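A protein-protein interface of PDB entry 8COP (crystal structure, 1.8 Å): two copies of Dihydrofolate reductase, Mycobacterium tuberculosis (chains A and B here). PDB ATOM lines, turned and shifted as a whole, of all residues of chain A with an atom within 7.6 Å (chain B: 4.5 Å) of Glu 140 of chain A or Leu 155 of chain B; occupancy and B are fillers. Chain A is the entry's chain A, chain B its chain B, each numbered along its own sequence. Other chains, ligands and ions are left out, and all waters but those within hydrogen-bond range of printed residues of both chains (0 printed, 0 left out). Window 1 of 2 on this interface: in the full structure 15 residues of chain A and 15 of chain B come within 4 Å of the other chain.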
ATOM      1  N   VAL A 114     -32.697  21.448  25.931  1.00  0.00           N
ATOM      2  CA  VAL A 114     -32.962  22.272  27.101  1.00  0.00           C
ATOM      3  C   VAL A 114     -33.829  23.453  26.700  1.00  0.00           C
ATOM      4  O   VAL A 114     -33.438  24.252  25.842  1.00  0.00           O
ATOM      5  CB  VAL A 114     -31.646  22.763  27.728  1.00  0.00           C
ATOM      6  CG1 VAL A 114     -31.910  23.551  28.996  1.00  0.00           C
ATOM      7  CG2 VAL A 114     -30.745  21.579  27.982  1.00  0.00           C
ATOM      8  N   ARG A 138     -21.143  20.215  23.361  1.00  0.00           N
ATOM      9  CA  ARG A 138     -21.237  21.324  22.419  1.00  0.00           C
ATOM     10  C   ARG A 138     -22.717  21.606  22.219  1.00  0.00           C
ATOM     11  O   ARG A 138     -23.508  20.674  22.067  1.00  0.00           O
ATOM     12  CB  ARG A 138     -20.576  20.974  21.081  1.00  0.00           C
ATOM     13  CG  ARG A 138     -19.043  20.839  21.139  1.00  0.00           C
ATOM     14  CD  ARG A 138     -18.442  20.417  19.791  1.00  0.00           C
ATOM     15  NE  ARG A 138     -18.430  21.483  18.785  1.00  0.00           N
ATOM     16  CZ  ARG A 138     -19.324  21.617  17.808  1.00  0.00           C
ATOM     17  NH1 ARG A 138     -20.334  20.762  17.704  1.00  0.00           N
ATOM     18  NH2 ARG A 138     -19.223  22.624  16.947  1.00  0.00           N
ATOM     19  N   GLY A 139     -23.107  22.881  22.282  1.00  0.00           N
ATOM     20  CA  GLY A 139     -24.543  23.197  22.155  1.00  0.00           C
ATOM     21  C   GLY A 139     -24.817  24.532  21.493  1.00  0.00           C
ATOM     22  O   GLY A 139     -24.085  25.496  21.764  1.00  0.00           O
ATOM     23  N   GLU A 140     -25.858  24.574  20.661  1.00  0.00           N
ATOM     24  CA  GLU A 140     -26.264  25.819  19.962  1.00  0.00           C
ATOM     25  C   GLU A 140     -27.319  26.528  20.818  1.00  0.00           C
ATOM     26  O   GLU A 140     -28.390  25.935  21.041  1.00  0.00           O
ATOM     27  CB  GLU A 140     -26.801  25.488  18.568  1.00  0.00           C
ATOM     28  CG  GLU A 140     -27.328  26.697  17.816  1.00  0.00           C
ATOM     29  CD  GLU A 140     -26.289  27.768  17.534  1.00  0.00           C
ATOM     30  OE1 GLU A 140     -25.636  28.223  18.493  1.00  0.00           O
ATOM     31  OE2 GLU A 140     -26.135  28.141  16.357  1.00  0.00           O
ATOM     32  N   THR A 141     -27.003  27.733  21.300  1.00  0.00           N
ATOM     33  CA  THR A 141     -27.955  28.522  22.124  1.00  0.00           C
ATOM     34  C   THR A 141     -29.016  29.122  21.197  1.00  0.00           C
ATOM     35  O   THR A 141     -28.711  29.316  20.009  1.00  0.00           O
ATOM     36  CB  THR A 141     -27.222  29.622  22.903  1.00  0.00           C
ATOM     37  OG1 THR A 141     -26.038  29.054  23.463  1.00  0.00           O
ATOM     38  CG2 THR A 141     -28.065  30.238  23.997  1.00  0.00           C
ATOM     39  N   GLY A 142     -30.216  29.383  21.720  1.00  0.00           N
ATOM     40  CA  GLY A 142     -31.267  29.974  20.918  1.00  0.00           C
ATOM     41  C   GLY A 142     -31.455  31.452  21.240  1.00  0.00           C
ATOM     42  O   GLY A 142     -30.742  32.038  22.052  1.00  0.00           O
ATOM     43  N   GLU A 143     -32.419  32.071  20.553  1.00  0.00           N
ATOM     44  CA  GLU A 143     -32.839  33.424  20.906  1.00  0.00           C
ATOM     45  C   GLU A 143     -34.112  33.370  21.735  1.00  0.00           C
ATOM     46  O   GLU A 143     -34.959  32.497  21.538  1.00  0.00           O
ATOM     47  CB  GLU A 143     -33.117  34.344  19.701  1.00  0.00           C
ATOM     48  CG  GLU A 143     -31.994  34.623  18.696  1.00  0.00           C
ATOM     49  CD  GLU A 143     -31.909  33.611  17.582  1.00  0.00           C
ATOM     50  OE1 GLU A 143     -31.461  34.018  16.487  1.00  0.00           O
ATOM     51  OE2 GLU A 143     -32.340  32.453  17.774  1.00  0.00           O
ATOM     52  N   ARG A 154     -35.847  30.076  25.591  1.00  0.00           N
ATOM     53  CA  ARG A 154     -35.133  29.733  24.368  1.00  0.00           C
ATOM     54  C   ARG A 154     -34.640  28.310  24.504  1.00  0.00           C
ATOM     55  O   ARG A 154     -34.374  27.838  25.612  1.00  0.00           O
ATOM     56  CB  ARG A 154     -33.983  30.709  24.082  1.00  0.00           C
ATOM     57  CG  ARG A 154     -33.149  31.081  25.271  1.00  0.00           C
ATOM     58  CD  ARG A 154     -31.774  31.493  24.864  1.00  0.00           C
ATOM     59  NE  ARG A 154     -30.941  31.826  26.012  1.00  0.00           N
ATOM     60  CZ  ARG A 154     -29.860  32.594  25.936  1.00  0.00           C
ATOM     61  NH1 ARG A 154     -29.548  33.184  24.789  1.00  0.00           N
ATOM     62  NH2 ARG A 154     -29.142  32.841  27.018  1.00  0.00           N
ATOM     63  N   LEU A 155     -34.569  27.620  23.377  1.00  0.00           N
ATOM     64  CA  LEU A 155     -34.175  26.229  23.428  1.00  0.00           C
ATOM     65  C   LEU A 155     -32.651  26.117  23.382  1.00  0.00           C
ATOM     66  O   LEU A 155     -31.926  27.074  23.101  1.00  0.00           O
ATOM     67  CB  LEU A 155     -34.837  25.445  22.297  1.00  0.00           C
ATOM     68  CG  LEU A 155     -36.335  25.712  22.113  1.00  0.00           C
ATOM     69  CD1 LEU A 155     -36.909  24.891  20.972  1.00  0.00           C
ATOM     70  CD2 LEU A 155     -37.144  25.495  23.366  1.00  0.00           C
ATOM     71  N   TYR A 156     -32.169  24.931  23.724  1.00  0.00           N
ATOM     72  CA  TYR A 156     -30.758  24.600  23.706  1.00  0.00           C
ATOM     73  C   TYR A 156     -30.709  23.154  23.284  1.00  0.00           C
ATOM     74  O   TYR A 156     -31.491  22.337  23.773  1.00  0.00           O
ATOM     75  CB  TYR A 156     -30.093  24.749  25.078  1.00  0.00           C
ATOM     76  CG  TYR A 156     -29.705  26.143  25.497  1.00  0.00           C
ATOM     77  CD1 TYR A 156     -28.395  26.594  25.402  1.00  0.00           C
ATOM     78  CD2 TYR A 156     -30.663  27.020  25.961  1.00  0.00           C
ATOM     79  CE1 TYR A 156     -28.057  27.876  25.799  1.00  0.00           C
ATOM     80  CE2 TYR A 156     -30.347  28.284  26.329  1.00  0.00           C
ATOM     81  CZ  TYR A 156     -29.053  28.720  26.263  1.00  0.00           C
ATOM     82  OH  TYR A 156     -28.792  30.014  26.672  1.00  0.00           O
ATOM     83  N   SER A 157     -29.820  22.841  22.363  1.00  0.00           N
ATOM     84  CA  SER A 157     -29.599  21.463  21.954  1.00  0.00           C
ATOM     85  C   SER A 157     -28.115  21.228  22.111  1.00  0.00           C
ATOM     86  O   SER A 157     -27.317  21.884  21.435  1.00  0.00           O
ATOM     87  CB  SER A 157     -30.055  21.216  20.515  1.00  0.00           C
ATOM     88  OG  SER A 157     -31.472  21.260  20.434  1.00  0.00           O
ATOM     89  N   TYR A 158     -27.754  20.352  23.046  1.00  0.00           N
ATOM     90  CA  TYR A 158     -26.374  19.951  23.269  1.00  0.00           C
ATOM     91  C   TYR A 158     -26.136  18.591  22.629  1.00  0.00           C
ATOM     92  O   TYR A 158     -27.035  17.750  22.556  1.00  0.00           O
ATOM     93  CB  TYR A 158     -26.024  19.898  24.764  1.00  0.00           C
ATOM     94  CG  TYR A 158     -26.081  21.237  25.484  1.00  0.00           C
ATOM     95  CD1 TYR A 158     -24.913  21.896  25.861  1.00  0.00           C
ATOM     96  CD2 TYR A 158     -27.301  21.814  25.842  1.00  0.00           C
ATOM     97  CE1 TYR A 158     -24.965  23.128  26.518  1.00  0.00           C
ATOM     98  CE2 TYR A 158     -27.360  23.033  26.507  1.00  0.00           C
ATOM     99  CZ  TYR A 158     -26.197  23.679  26.840  1.00  0.00           C
ATOM    100  OH  TYR A 158     -26.261  24.885  27.498  1.00  0.00           O
ATOM    101  N   HIS A 159     -24.925  18.403  22.118  1.00  0.00           N
ATOM    102  CA  HIS A 159     -24.548  17.110  21.577  1.00  0.00           C
ATOM    103  C   HIS A 159     -23.084  16.883  21.865  1.00  0.00           C
ATOM    104  O   HIS A 159     -22.285  17.820  21.888  1.00  0.00           O
ATOM    105  CB  HIS A 159     -24.817  16.983  20.065  1.00  0.00           C
ATOM    106  CG  HIS A 159     -24.501  15.623  19.496  1.00  0.00           C
ATOM    107  ND1 HIS A 159     -23.211  15.162  19.321  1.00  0.00           N
ATOM    108  CD2 HIS A 159     -25.314  14.607  19.106  1.00  0.00           C
ATOM    109  CE1 HIS A 159     -23.244  13.935  18.820  1.00  0.00           C
ATOM    110  NE2 HIS A 159     -24.507  13.570  18.690  1.00  0.00           N
ATOM    111  N   HIS B  32     -19.128  20.956  13.473  1.00  0.00           N
ATOM    112  CA  HIS B  32     -20.531  20.587  13.640  1.00  0.00           C
ATOM    113  C   HIS B  32     -20.829  19.263  12.951  1.00  0.00           C
ATOM    114  O   HIS B  32     -21.324  18.328  13.573  1.00  0.00           O
ATOM    115  CB  HIS B  32     -21.443  21.680  13.103  1.00  0.00           C
ATOM    116  CG  HIS B  32     -22.897  21.390  13.296  1.00  0.00           C
ATOM    117  ND1 HIS B  32     -23.698  20.869  12.303  1.00  0.00           N
ATOM    118  CD2 HIS B  32     -23.699  21.550  14.375  1.00  0.00           C
ATOM    119  CE1 HIS B  32     -24.928  20.723  12.760  1.00  0.00           C
ATOM    120  NE2 HIS B  32     -24.956  21.138  14.014  1.00  0.00           N
ATOM    121  N   VAL B 114     -29.608  21.012   9.307  1.00  0.00           N
ATOM    122  CA  VAL B 114     -29.320  21.931   8.213  1.00  0.00           C
ATOM    123  C   VAL B 114     -28.419  23.046   8.714  1.00  0.00           C
ATOM    124  O   VAL B 114     -28.658  23.623   9.781  1.00  0.00           O
ATOM    125  CB  VAL B 114     -30.612  22.506   7.604  1.00  0.00           C
ATOM    126  CG1 VAL B 114     -30.307  23.359   6.378  1.00  0.00           C
ATOM    127  CG2 VAL B 114     -31.562  21.384   7.235  1.00  0.00           C
ATOM    128  N   THR B 115     -27.390  23.340   7.935  1.00  0.00           N
ATOM    129  CA  THR B 115     -26.597  24.549   8.039  1.00  0.00           C
ATOM    130  C   THR B 115     -26.993  25.470   6.884  1.00  0.00           C
ATOM    131  O   THR B 115     -27.279  24.995   5.781  1.00  0.00           O
ATOM    132  CB  THR B 115     -25.116  24.187   7.965  1.00  0.00           C
ATOM    133  OG1 THR B 115     -24.779  23.290   9.040  1.00  0.00           O
ATOM    134  CG2 THR B 115     -24.244  25.427   8.005  1.00  0.00           C
ATOM    135  N   GLU B 140     -36.366  23.704  14.710  1.00  0.00           N
ATOM    136  CA  GLU B 140     -35.949  24.751  15.633  1.00  0.00           C
ATOM    137  C   GLU B 140     -34.666  25.380  15.116  1.00  0.00           C
ATOM    138  O   GLU B 140     -33.649  24.695  14.959  1.00  0.00           O
ATOM    139  CB  GLU B 140     -35.794  24.196  17.056  1.00  0.00           C
ATOM    140  CG  GLU B 140     -36.992  23.346  17.511  1.00  0.00           C
ATOM    141  CD  GLU B 140     -38.215  24.207  17.878  1.00  0.00           C
ATOM    142  OE1 GLU B 140     -38.309  25.385  17.458  1.00  0.00           O
ATOM    143  OE2 GLU B 140     -39.137  23.671  18.523  1.00  0.00           O
ATOM    144  N   THR B 141     -34.730  26.681  14.844  1.00  0.00           N
ATOM    145  CA  THR B 141     -33.656  27.378  14.156  1.00  0.00           C
ATOM    146  C   THR B 141     -32.490  27.577  15.113  1.00  0.00           C
ATOM    147  O   THR B 141     -31.881  26.602  15.567  1.00  0.00           O
ATOM    148  CB  THR B 141     -34.167  28.706  13.593  1.00  0.00           C
ATOM    149  OG1 THR B 141     -35.294  28.440  12.750  1.00  0.00           O
ATOM    150  CG2 THR B 141     -33.110  29.377  12.740  1.00  0.00           C
ATOM    151  N   GLY B 142     -32.201  28.810  15.467  1.00  0.00           N
ATOM    152  CA  GLY B 142     -30.967  29.153  16.145  1.00  0.00           C
ATOM    153  C   GLY B 142     -30.441  30.473  15.619  1.00  0.00           C
ATOM    154  O   GLY B 142     -30.874  30.990  14.588  1.00  0.00           O
ATOM    155  N   GLU B 143     -29.482  31.024  16.344  1.00  0.00           N
ATOM    156  CA  GLU B 143     -29.005  32.370  16.087  1.00  0.00           C
ATOM    157  C   GLU B 143     -28.113  32.430  14.842  1.00  0.00           C
ATOM    158  O   GLU B 143     -27.460  31.446  14.484  1.00  0.00           O
ATOM    159  CB  GLU B 143     -28.304  32.870  17.355  1.00  0.00           C
ATOM    160  CG  GLU B 143     -27.081  32.048  17.785  1.00  0.00           C
ATOM    161  CD  GLU B 143     -26.496  32.530  19.112  1.00  0.00           C
ATOM    162  OE1 GLU B 143     -27.048  33.504  19.663  1.00  0.00           O
ATOM    163  OE2 GLU B 143     -25.514  31.931  19.617  1.00  0.00           O
ATOM    164  N   ARG B 145     -25.075  32.828  13.526  1.00  0.00           N
ATOM    165  CA  ARG B 145     -23.715  32.729  14.004  1.00  0.00           C
ATOM    166  C   ARG B 145     -22.776  33.542  13.110  1.00  0.00           C
ATOM    167  O   ARG B 145     -23.136  33.985  12.020  1.00  0.00           O
ATOM    168  CB  ARG B 145     -23.326  31.259  14.044  1.00  0.00           C
ATOM    169  CG  ARG B 145     -24.194  30.377  14.961  1.00  0.00           C
ATOM    170  CD  ARG B 145     -23.941  30.636  16.428  1.00  0.00           C
ATOM    171  NE  ARG B 145     -22.589  30.177  16.752  1.00  0.00           N
ATOM    172  CZ  ARG B 145     -21.907  30.498  17.846  1.00  0.00           C
ATOM    173  NH1 ARG B 145     -22.449  31.283  18.772  1.00  0.00           N
ATOM    174  NH2 ARG B 145     -20.679  30.018  18.023  1.00  0.00           N
ATOM    175  N   ARG B 154     -26.334  29.983  10.024  1.00  0.00           N
ATOM    176  CA  ARG B 154     -27.167  29.606  11.148  1.00  0.00           C
ATOM    177  C   ARG B 154     -27.461  28.116  11.075  1.00  0.00           C
ATOM    178  O   ARG B 154     -27.362  27.490  10.017  1.00  0.00           O
ATOM    179  CB  ARG B 154     -28.461  30.424  11.202  1.00  0.00           C
ATOM    180  CG  ARG B 154     -29.533  30.070  10.182  1.00  0.00           C
ATOM    181  CD  ARG B 154     -30.788  30.875  10.519  1.00  0.00           C
ATOM    182  NE  ARG B 154     -31.746  31.022   9.428  1.00  0.00           N
ATOM    183  CZ  ARG B 154     -32.688  31.961   9.393  1.00  0.00           C
ATOM    184  NH1 ARG B 154     -32.802  32.839  10.379  1.00  0.00           N
ATOM    185  NH2 ARG B 154     -33.528  32.002   8.373  1.00  0.00           N
ATOM    186  N   LEU B 155     -27.786  27.545  12.230  1.00  0.00           N
ATOM    187  CA  LEU B 155     -28.089  26.127  12.342  1.00  0.00           C
ATOM    188  C   LEU B 155     -29.589  25.924  12.404  1.00  0.00           C
ATOM    189  O   LEU B 155     -30.311  26.718  13.012  1.00  0.00           O
ATOM    190  CB  LEU B 155     -27.420  25.510  13.573  1.00  0.00           C
ATOM    191  CG  LEU B 155     -25.896  25.561  13.506  1.00  0.00           C
ATOM    192  CD1 LEU B 155     -25.222  24.825  14.640  1.00  0.00           C
ATOM    193  CD2 LEU B 155     -25.492  24.929  12.185  1.00  0.00           C
ATOM    194  N   TYR B 156     -30.046  24.872  11.732  1.00  0.00           N
ATOM    195  CA  TYR B 156     -31.400  24.365  11.843  1.00  0.00           C
ATOM    196  C   TYR B 156     -31.337  22.924  12.300  1.00  0.00           C
ATOM    197  O   TYR B 156     -30.450  22.174  11.893  1.00  0.00           O
ATOM    198  CB  TYR B 156     -32.139  24.408  10.511  1.00  0.00           C
ATOM    199  CG  TYR B 156     -32.472  25.769   9.984  1.00  0.00           C
ATOM    200  CD1 TYR B 156     -31.574  26.455   9.195  1.00  0.00           C
ATOM    201  CD2 TYR B 156     -33.715  26.335  10.213  1.00  0.00           C
ATOM    202  CE1 TYR B 156     -31.878  27.692   8.691  1.00  0.00           C
ATOM    203  CE2 TYR B 156     -34.037  27.565   9.710  1.00  0.00           C
ATOM    204  CZ  TYR B 156     -33.110  28.243   8.947  1.00  0.00           C
ATOM    205  OH  TYR B 156     -33.394  29.482   8.415  1.00  0.00           O
ATOM    206  N   SER B 157     -32.290  22.532  13.131  1.00  0.00           N
ATOM    207  CA  SER B 157     -32.505  21.129  13.441  1.00  0.00           C
ATOM    208  C   SER B 157     -33.978  20.837  13.198  1.00  0.00           C
ATOM    209  O   SER B 157     -34.850  21.495  13.772  1.00  0.00           O
ATOM    210  CB  SER B 157     -32.070  20.804  14.879  1.00  0.00           C
ATOM    211  OG  SER B 157     -33.082  21.053  15.832  1.00  0.00           O
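The backbone carbonyl oxygen (O) of Ser 157 of chain A sits at hydrogen-bond distance from the backbone NH (N) of Glu 140 of chain A (3.2 Å). N of Glu 140 of chain B is in hydrogen-bond range of O of Ser 157 of chain B (2.8 Å). The guanidinium group of Arg 145 of chain B lies within salt-bridge range of the side-chain carboxylate of Glu 143 of chain B, at 3.2 Å. N of Gly 142 of chain A sits at hydrogen-bond distance from O of Leu 155 of chain A (3.2 Å). O of Arg 138 of chain A lies within hydrogen-bond range of N of His 159 of chain A.
N of His 32 of chain B touches NH2 of Arg 138 of chain A (3.9 Å). Glu 140 of chain A touches Glu 143 of chain B. Glu 140 of chain A touches Arg 145 of chain B (OE2 to CG, 3.3 Å). Leu 155 of chain B touches Glu 140 of chain A. Thr 141 of chain A touches Glu 143 of chain B (O to CG, 3.9 Å). Gly 142 of chain B touches Glu 143 of chain A (C to OE2, 3.5 Å). Glu 143 of chain A touches Glu 143 of chain B. Glu 140 of chain B touches Leu 155 of chain A.
Printed residues of chain B within 4 Å of Arg 138 of chain A: His 32 (3.9 Å). Glu 140 of chain A touches just these residues of chain B: Glu 143, Arg 145 and Leu 155. Of the printed residues of chain B, Thr 141 of chain A touches Glu 143. Printed residues of chain B within 4 Å of Leu 155 of chain A: Glu 140 (3.4 Å). Of the printed residues of chain A, Glu 140 of chain B touches Leu 155. Of the printed residues of chain A, Glu 143 of chain B touches Glu 140 (3.9 Å), Thr 141 (3.9 Å) and Glu 143 (3.0 Å). Printed residues of chain A within 4 Å of Leu 155 of chain B: Glu 140 (3.8 Å). The nearest printed residue of chain B that does not touch Thr 141 of chain A is Gly 142 of chain B (4.5 Å).
Hydrophobic or aromatic side chains of chain B that line the printed part of chain A: Leu 155. Of the 13 printed residues of chain A, 5 touch a printed residue of chain B. Hydrophobic or aromatic side chains of chain A within 4 Å of the printed part of chain B: Leu 155. Among the printed residues, 8 pairs touch across the chains.
Glu 140 of chain A touches Glu 143 of chain B, but with the chains exchanged Glu 143 of chain A does not touch Glu 140 of chain B (7.9 Å). Glu 140 of chain A touches Leu 155 of chain B, and with the chains exchanged Leu 155 of chain A touches Glu 140 of chain B. Thr 141 of chain A touches Glu 143 of chain B, but with the chains exchanged Glu 143 of chain A does not touch Thr 141 of chain B (5.6 Å). Glu 143 of chain A touches Gly 142 of chain B, but with the chains exchanged Gly 142 of chain A does not touch Glu 143 of chain B (4.6 Å). 9 positions are printed for both chains.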
